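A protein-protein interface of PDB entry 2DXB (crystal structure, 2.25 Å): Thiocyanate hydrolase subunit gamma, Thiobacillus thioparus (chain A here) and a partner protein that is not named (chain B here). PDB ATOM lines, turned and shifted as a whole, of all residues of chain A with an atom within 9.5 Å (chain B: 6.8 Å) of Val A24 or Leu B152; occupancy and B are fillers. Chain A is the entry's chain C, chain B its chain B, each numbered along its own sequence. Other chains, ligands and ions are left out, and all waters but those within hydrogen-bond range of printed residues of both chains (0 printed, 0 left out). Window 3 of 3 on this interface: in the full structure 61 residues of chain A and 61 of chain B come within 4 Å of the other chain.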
ATOM      1  N   GLU A  23      22.255 -15.409  21.571  1.00  0.00           N
ATOM      2  CA  GLU A  23      23.313 -15.060  20.580  1.00  0.00           C
ATOM      3  C   GLU A  23      24.146 -16.268  20.178  1.00  0.00           C
ATOM      4  O   GLU A  23      24.409 -17.157  20.986  1.00  0.00           O
ATOM      5  CB  GLU A  23      24.253 -13.990  21.148  1.00  0.00           C
ATOM      6  CG  GLU A  23      23.642 -12.607  21.267  1.00  0.00           C
ATOM      7  CD  GLU A  23      24.655 -11.566  21.708  1.00  0.00           C
ATOM      8  OE1 GLU A  23      25.240 -11.728  22.802  1.00  0.00           O
ATOM      9  OE2 GLU A  23      24.869 -10.587  20.960  1.00  0.00           O
ATOM     10  N   VAL A  24      24.552 -16.289  18.916  1.00  0.00           N
ATOM     11  CA  VAL A  24      25.386 -17.352  18.389  1.00  0.00           C
ATOM     12  C   VAL A  24      26.724 -16.694  18.077  1.00  0.00           C
ATOM     13  O   VAL A  24      26.779 -15.494  17.808  1.00  0.00           O
ATOM     14  CB  VAL A  24      24.782 -17.956  17.103  1.00  0.00           C
ATOM     15  CG1 VAL A  24      23.443 -18.598  17.419  1.00  0.00           C
ATOM     16  CG2 VAL A  24      24.607 -16.876  16.050  1.00  0.00           C
ATOM     17  N   SER A  25      27.800 -17.466  18.129  1.00  0.00           N
ATOM     18  CA  SER A  25      29.126 -16.929  17.857  1.00  0.00           C
ATOM     19  C   SER A  25      29.417 -16.926  16.361  1.00  0.00           C
ATOM     20  O   SER A  25      28.669 -17.503  15.571  1.00  0.00           O
ATOM     21  CB  SER A  25      30.187 -17.767  18.566  1.00  0.00           C
ATOM     22  OG  SER A  25      30.257 -19.060  17.990  1.00  0.00           O
ATOM     23  N   ASP A  26      30.513 -16.275  15.979  1.00  0.00           N
ATOM     24  CA  ASP A  26      30.922 -16.212  14.580  1.00  0.00           C
ATOM     25  C   ASP A  26      31.320 -17.608  14.115  1.00  0.00           C
ATOM     26  O   ASP A  26      31.206 -17.935  12.932  1.00  0.00           O
ATOM     27  CB  ASP A  26      32.111 -15.261  14.418  1.00  0.00           C
ATOM     28  CG  ASP A  26      31.735 -13.813  14.640  1.00  0.00           C
ATOM     29  OD1 ASP A  26      30.963 -13.271  13.823  1.00  0.00           O
ATOM     30  OD2 ASP A  26      32.206 -13.216  15.628  1.00  0.00           O
ATOM     31  N   PHE A  27      31.796 -18.426  15.051  1.00  0.00           N
ATOM     32  CA  PHE A  27      32.209 -19.787  14.733  1.00  0.00           C
ATOM     33  C   PHE A  27      30.995 -20.619  14.350  1.00  0.00           C
ATOM     34  O   PHE A  27      31.033 -21.381  13.384  1.00  0.00           O
ATOM     35  CB  PHE A  27      32.909 -20.429  15.935  1.00  0.00           C
ATOM     36  CG  PHE A  27      34.192 -19.750  16.328  1.00  0.00           C
ATOM     37  CD1 PHE A  27      35.323 -19.842  15.520  1.00  0.00           C
ATOM     38  CD2 PHE A  27      34.276 -19.036  17.519  1.00  0.00           C
ATOM     39  CE1 PHE A  27      36.521 -19.238  15.898  1.00  0.00           C
ATOM     40  CE2 PHE A  27      35.475 -18.424  17.902  1.00  0.00           C
ATOM     41  CZ  PHE A  27      36.596 -18.528  17.090  1.00  0.00           C
ATOM     42  N   GLU A  28      29.916 -20.471  15.111  1.00  0.00           N
ATOM     43  CA  GLU A  28      28.694 -21.217  14.834  1.00  0.00           C
ATOM     44  C   GLU A  28      28.070 -20.754  13.524  1.00  0.00           C
ATOM     45  O   GLU A  28      27.545 -21.565  12.765  1.00  0.00           O
ATOM     46  CB  GLU A  28      27.724 -21.070  16.010  1.00  0.00           C
ATOM     47  CG  GLU A  28      28.347 -21.605  17.293  1.00  0.00           C
ATOM     48  CD  GLU A  28      27.527 -21.345  18.532  1.00  0.00           C
ATOM     49  OE1 GLU A  28      26.951 -20.241  18.648  1.00  0.00           O
ATOM     50  OE2 GLU A  28      27.479 -22.243  19.399  1.00  0.00           O
ATOM     51  N   ILE A  29      28.142 -19.456  13.245  1.00  0.00           N
ATOM     52  CA  ILE A  29      27.601 -18.938  11.993  1.00  0.00           C
ATOM     53  C   ILE A  29      28.380 -19.558  10.831  1.00  0.00           C
ATOM     54  O   ILE A  29      27.795 -20.085   9.880  1.00  0.00           O
ATOM     55  CB  ILE A  29      27.747 -17.403  11.891  1.00  0.00           C
ATOM     56  CG1 ILE A  29      26.715 -16.704  12.781  1.00  0.00           C
ATOM     57  CG2 ILE A  29      27.607 -16.970  10.437  1.00  0.00           C
ATOM     58  CD1 ILE A  29      25.282 -16.859  12.305  1.00  0.00           C
ATOM     59  N   LEU A  30      29.705 -19.491  10.918  1.00  0.00           N
ATOM     60  CA  LEU A  30      30.566 -20.024   9.869  1.00  0.00           C
ATOM     61  C   LEU A  30      30.451 -21.539   9.726  1.00  0.00           C
ATOM     62  O   LEU A  30      30.493 -22.061   8.613  1.00  0.00           O
ATOM     63  CB  LEU A  30      32.024 -19.634  10.131  1.00  0.00           C
ATOM     64  CG  LEU A  30      33.062 -20.052   9.080  1.00  0.00           C
ATOM     65  CD1 LEU A  30      32.676 -19.502   7.704  1.00  0.00           C
ATOM     66  CD2 LEU A  30      34.431 -19.532   9.497  1.00  0.00           C
ATOM     67  N   GLU A  31      30.315 -22.243  10.846  1.00  0.00           N
ATOM     68  CA  GLU A  31      30.191 -23.699  10.817  1.00  0.00           C
ATOM     69  C   GLU A  31      28.949 -24.077  10.005  1.00  0.00           C
ATOM     70  O   GLU A  31      28.996 -24.973   9.160  1.00  0.00           O
ATOM     71  CB  GLU A  31      30.093 -24.246  12.248  1.00  0.00           C
ATOM     72  CG  GLU A  31      30.168 -25.767  12.373  1.00  0.00           C
ATOM     73  CD  GLU A  31      28.900 -26.465  11.903  1.00  0.00           C
ATOM     74  OE1 GLU A  31      27.798 -26.070  12.345  1.00  0.00           O
ATOM     75  OE2 GLU A  31      29.005 -27.415  11.098  1.00  0.00           O
ATOM     76  N   MET A  32      27.839 -23.389  10.263  1.00  0.00           N
ATOM     77  CA  MET A  32      26.595 -23.639   9.534  1.00  0.00           C
ATOM     78  C   MET A  32      26.797 -23.355   8.045  1.00  0.00           C
ATOM     79  O   MET A  32      26.372 -24.130   7.188  1.00  0.00           O
ATOM     80  CB  MET A  32      25.477 -22.740  10.070  1.00  0.00           C
ATOM     81  CG  MET A  32      24.847 -23.220  11.371  1.00  0.00           C
ATOM     82  SD  MET A  32      23.730 -24.626  11.112  1.00  0.00           S
ATOM     83  CE  MET A  32      22.274 -23.756  10.484  1.00  0.00           C
ATOM     84  N   ASN A 236      30.880 -22.656  25.768  1.00  0.00           N
ATOM     85  CA  ASN A 236      29.726 -21.774  25.728  1.00  0.00           C
ATOM     86  C   ASN A 236      28.464 -22.594  25.466  1.00  0.00           C
ATOM     87  O   ASN A 236      27.459 -22.440  26.158  1.00  0.00           O
ATOM     88  CB  ASN A 236      29.907 -20.727  24.631  1.00  0.00           C
ATOM     89  CG  ASN A 236      28.707 -19.810  24.498  1.00  0.00           C
ATOM     90  OD1 ASN A 236      28.313 -19.138  25.457  1.00  0.00           O
ATOM     91  ND2 ASN A 236      28.117 -19.775  23.304  1.00  0.00           N
ATOM     92  N   ARG A 237      28.527 -23.472  24.471  1.00  0.00           N
ATOM     93  CA  ARG A 237      27.397 -24.322  24.112  1.00  0.00           C
ATOM     94  C   ARG A 237      27.915 -25.746  23.903  1.00  0.00           C
ATOM     95  O   ARG A 237      28.113 -26.188  22.774  1.00  0.00           O
ATOM     96  CB  ARG A 237      26.748 -23.789  22.833  1.00  0.00           C
ATOM     97  CG  ARG A 237      25.487 -24.517  22.409  1.00  0.00           C
ATOM     98  CD  ARG A 237      24.992 -24.037  21.046  1.00  0.00           C
ATOM     99  NE  ARG A 237      24.252 -22.778  21.104  1.00  0.00           N
ATOM    100  CZ  ARG A 237      24.798 -21.577  21.263  1.00  0.00           C
ATOM    101  NH1 ARG A 237      26.109 -21.448  21.381  1.00  0.00           N
ATOM    102  NH2 ARG A 237      24.028 -20.499  21.308  1.00  0.00           N
ATOM    103  N   MET B 138      23.105 -16.712   6.795  1.00  0.00           N
ATOM    104  CA  MET B 138      23.109 -17.292   8.129  1.00  0.00           C
ATOM    105  C   MET B 138      22.795 -16.234   9.189  1.00  0.00           C
ATOM    106  O   MET B 138      22.041 -16.488  10.131  1.00  0.00           O
ATOM    107  CB  MET B 138      24.466 -17.944   8.396  1.00  0.00           C
ATOM    108  CG  MET B 138      24.380 -19.377   8.888  1.00  0.00           C
ATOM    109  SD  MET B 138      23.334 -20.459   7.871  1.00  0.00           S
ATOM    110  CE  MET B 138      24.487 -21.002   6.684  1.00  0.00           C
ATOM    111  N   ARG B 141      19.173 -15.185   9.013  1.00  0.00           N
ATOM    112  CA  ARG B 141      18.364 -16.265   9.562  1.00  0.00           C
ATOM    113  C   ARG B 141      18.223 -16.082  11.077  1.00  0.00           C
ATOM    114  O   ARG B 141      17.131 -16.211  11.630  1.00  0.00           O
ATOM    115  CB  ARG B 141      19.016 -17.614   9.237  1.00  0.00           C
ATOM    116  CG  ARG B 141      18.109 -18.818   9.422  1.00  0.00           C
ATOM    117  CD  ARG B 141      18.822 -20.131   9.085  1.00  0.00           C
ATOM    118  NE  ARG B 141      19.018 -20.333   7.649  1.00  0.00           N
ATOM    119  CZ  ARG B 141      19.667 -21.371   7.124  1.00  0.00           C
ATOM    120  NH1 ARG B 141      20.187 -22.302   7.914  1.00  0.00           N
ATOM    121  NH2 ARG B 141      19.794 -21.485   5.809  1.00  0.00           N
ATOM    122  N   VAL B 142      19.327 -15.756  11.743  1.00  0.00           N
ATOM    123  CA  VAL B 142      19.316 -15.549  13.188  1.00  0.00           C
ATOM    124  C   VAL B 142      18.591 -14.256  13.556  1.00  0.00           C
ATOM    125  O   VAL B 142      17.816 -14.219  14.512  1.00  0.00           O
ATOM    126  CB  VAL B 142      20.753 -15.484  13.761  1.00  0.00           C
ATOM    127  CG1 VAL B 142      20.718 -15.078  15.223  1.00  0.00           C
ATOM    128  CG2 VAL B 142      21.428 -16.836  13.617  1.00  0.00           C
ATOM    129  N   ALA B 143      18.846 -13.202  12.788  1.00  0.00           N
ATOM    130  CA  ALA B 143      18.238 -11.900  13.035  1.00  0.00           C
ATOM    131  C   ALA B 143      16.721 -11.895  12.902  1.00  0.00           C
ATOM    132  O   ALA B 143      16.046 -11.089  13.537  1.00  0.00           O
ATOM    133  CB  ALA B 143      18.841 -10.863  12.098  1.00  0.00           C
ATOM    134  N   GLY B 145      14.793 -14.327  13.807  1.00  0.00           N
ATOM    135  CA  GLY B 145      14.248 -15.315  14.721  1.00  0.00           C
ATOM    136  C   GLY B 145      13.938 -16.642  14.058  1.00  0.00           C
ATOM    137  O   GLY B 145      13.163 -17.445  14.579  1.00  0.00           O
ATOM    138  N   GLN B 146      14.551 -16.880  12.906  1.00  0.00           N
ATOM    139  CA  GLN B 146      14.338 -18.117  12.169  1.00  0.00           C
ATOM    140  C   GLN B 146      15.241 -19.234  12.706  1.00  0.00           C
ATOM    141  O   GLN B 146      15.217 -20.358  12.209  1.00  0.00           O
ATOM    142  CB  GLN B 146      14.607 -17.867  10.686  1.00  0.00           C
ATOM    143  CG  GLN B 146      14.054 -18.917   9.751  1.00  0.00           C
ATOM    144  CD  GLN B 146      13.916 -18.389   8.337  1.00  0.00           C
ATOM    145  OE1 GLN B 146      13.163 -17.444   8.089  1.00  0.00           O
ATOM    146  NE2 GLN B 146      14.646 -18.990   7.403  1.00  0.00           N
ATOM    147  N   GLY B 147      16.034 -18.911  13.724  1.00  0.00           N
ATOM    148  CA  GLY B 147      16.925 -19.891  14.325  1.00  0.00           C
ATOM    149  C   GLY B 147      18.145 -20.266  13.500  1.00  0.00           C
ATOM    150  O   GLY B 147      18.288 -19.842  12.351  1.00  0.00           O
ATOM    151  N   LEU B 148      19.028 -21.066  14.093  1.00  0.00           N
ATOM    152  CA  LEU B 148      20.245 -21.510  13.421  1.00  0.00           C
ATOM    153  C   LEU B 148      20.635 -22.922  13.857  1.00  0.00           C
ATOM    154  O   LEU B 148      21.359 -23.093  14.839  1.00  0.00           O
ATOM    155  CB  LEU B 148      21.401 -20.548  13.725  1.00  0.00           C
ATOM    156  CG  LEU B 148      22.701 -20.797  12.954  1.00  0.00           C
ATOM    157  CD1 LEU B 148      22.515 -20.355  11.513  1.00  0.00           C
ATOM    158  CD2 LEU B 148      23.851 -20.031  13.590  1.00  0.00           C
ATOM    159  N   GLY B 149      20.158 -23.925  13.124  1.00  0.00           N
ATOM    160  CA  GLY B 149      20.473 -25.308  13.452  1.00  0.00           C
ATOM    161  C   GLY B 149      20.225 -25.645  14.912  1.00  0.00           C
ATOM    162  O   GLY B 149      19.243 -25.189  15.496  1.00  0.00           O
ATOM    163  N   GLU B 150      21.125 -26.445  15.491  1.00  0.00           N
ATOM    164  CA  GLU B 150      20.863 -26.788  16.883  1.00  0.00           C
ATOM    165  C   GLU B 150      21.659 -25.893  17.826  1.00  0.00           C
ATOM    166  O   GLU B 150      21.752 -26.016  19.031  1.00  0.00           O
ATOM    167  CB  GLU B 150      21.212 -28.255  17.144  1.00  0.00           C
ATOM    168  CG  GLU B 150      22.080 -28.479  18.371  1.00  0.00           C
ATOM    169  CD  GLU B 150      22.625 -29.890  18.451  1.00  0.00           C
ATOM    170  OE1 GLU B 150      23.364 -30.298  17.530  1.00  0.00           O
ATOM    171  OE2 GLU B 150      22.314 -30.594  19.435  1.00  0.00           O
ATOM    172  N   TYR B 151      22.067 -24.682  17.255  1.00  0.00           N
ATOM    173  CA  TYR B 151      22.720 -23.640  18.036  1.00  0.00           C
ATOM    174  C   TYR B 151      21.683 -22.683  18.608  1.00  0.00           C
ATOM    175  O   TYR B 151      21.817 -22.199  19.732  1.00  0.00           O
ATOM    176  CB  TYR B 151      23.695 -22.854  17.159  1.00  0.00           C
ATOM    177  CG  TYR B 151      24.779 -23.698  16.535  1.00  0.00           C
ATOM    178  CD1 TYR B 151      24.900 -23.797  15.150  1.00  0.00           C
ATOM    179  CD2 TYR B 151      25.682 -24.404  17.330  1.00  0.00           C
ATOM    180  CE1 TYR B 151      25.897 -24.579  14.569  1.00  0.00           C
ATOM    181  CE2 TYR B 151      26.677 -25.188  16.760  1.00  0.00           C
ATOM    182  CZ  TYR B 151      26.778 -25.272  15.381  1.00  0.00           C
ATOM    183  OH  TYR B 151      27.752 -26.062  14.817  1.00  0.00           O
ATOM    184  N   LEU B 152      20.647 -22.416  17.822  1.00  0.00           N
ATOM    185  CA  LEU B 152      19.598 -21.499  18.232  1.00  0.00           C
ATOM    186  C   LEU B 152      18.238 -21.935  17.699  1.00  0.00           C
ATOM    187  O   LEU B 152      18.041 -22.055  16.487  1.00  0.00           O
ATOM    188  CB  LEU B 152      19.917 -20.094  17.722  1.00  0.00           C
ATOM    189  CG  LEU B 152      18.923 -19.000  18.106  1.00  0.00           C
ATOM    190  CD1 LEU B 152      18.955 -18.801  19.614  1.00  0.00           C
ATOM    191  CD2 LEU B 152      19.273 -17.708  17.387  1.00  0.00           C
ATOM    192  N   PRO B 153      17.277 -22.186  18.601  1.00  0.00           N
ATOM    193  CA  PRO B 153      15.939 -22.604  18.177  1.00  0.00           C
ATOM    194  C   PRO B 153      15.162 -21.394  17.666  1.00  0.00           C
ATOM    195  O   PRO B 153      15.362 -20.275  18.140  1.00  0.00           O
ATOM    196  CB  PRO B 153      15.343 -23.175  19.457  1.00  0.00           C
ATOM    197  CG  PRO B 153      15.937 -22.282  20.507  1.00  0.00           C
ATOM    198  CD  PRO B 153      17.389 -22.189  20.071  1.00  0.00           C
ATOM    199  N   PRO B 154      14.277 -21.596  16.678  1.00  0.00           N
ATOM    200  CA  PRO B 154      13.518 -20.450  16.172  1.00  0.00           C
ATOM    201  C   PRO B 154      12.552 -19.908  17.228  1.00  0.00           C
ATOM    202  O   PRO B 154      12.295 -20.634  18.215  1.00  0.00           O
ATOM    203  CB  PRO B 154      12.799 -21.028  14.955  1.00  0.00           C
ATOM    204  CG  PRO B 154      12.602 -22.467  15.332  1.00  0.00           C
ATOM    205  CD  PRO B 154      13.931 -22.829  15.950  1.00  0.00           C
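Among the printed residues, merely in contact across the chains: Met A32 with Gly B149 (3.4 Å), Glu A28 with Tyr B151 (3.5 Å), Met A32 with Leu B148 (3.6 Å), Met A32 with Met B138 (3.6 Å), Met A32 with Arg B141 (3.6 Å), Ile A29 with Met B138 (3.6 Å), Met A32 with Tyr B151 (3.6 Å), Ile A29 with Leu B148 (3.7 Å) and Val A24 with Leu B152 (3.8 Å).
OE1 of Glu A31 sits at hydrogen-bond distance from OH of Tyr B151, at 2.5 Å.
The guanidinium group (NE) of Arg A237 is in hydrogen-bond range of the backbone carbonyl oxygen (O) of Tyr B151 (2.9 Å).
The side-chain sulfur (SD) of Met B138 lies within hydrogen-bond range of the guanidinium group (NH1) of Arg B141 (3.6 Å).
O of Arg B141 sits at hydrogen-bond distance from N of Gln B146 (3.0 Å).
The backbone carbonyl oxygen of Glu A23 is in hydrogen-bond range of the guanidinium group of Arg A237, at 3.4 Å.
The backbone NH of Ser A25 lies within hydrogen-bond range of the side-chain carboxylate of Glu A28 (2.9 Å).
OE2 of Glu A28 lies within salt-bridge range of NH1 of Arg A237 (2.5 Å).
NH1 of Arg A237 lies close to ND2 of Asn A236 (3.2 Å).
Printed residues of chain A that touch a printed residue of chain B: Val A24, Glu A28, Ile A29, Glu A31, Met A32 and Arg A237.
Along chain A the printed residues that touch a printed residue of chain B span positions 24 to 237.
Of the 14 printed residues of chain B, 6 touch a printed residue of chain A.
Hydrophobic or aromatic side chains of chain B within 4 Å of the printed part of chain A: Met B138, Leu B148, Tyr B151 and Leu B152.
Among the printed residues, 11 pairs touch across the chains.
Among the printed residues, no Asp or Glu carboxylate lies within 4 Å of a Lys or Arg side-chain nitrogen of the other chain.
Of chain A, only Val A24 (3.8 Å) comes within 4 Å of Leu B152.
No residue of chain A comes within 4 Å of Pro B153.
Of the printed residues of chain B, Glu A28 touches Tyr B151 (3.5 Å).
Of the printed residues of chain A, Arg B141 touches Met A32 (3.6 Å).
Of the printed residues of chain A, Met B138 touches Ile A29 (3.6 Å) and Met A32 (3.6 Å).
Leu A30 touches none of the printed residues of chain B.
Gly B145 touches none of the printed residues of chain A.
The nearest printed residue of chain B that does not touch Val A24 is Val B142 (4.003 Å).
The nearest printed residue of chain B that does not touch Ile A29 is Val B142 (4.1 Å).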
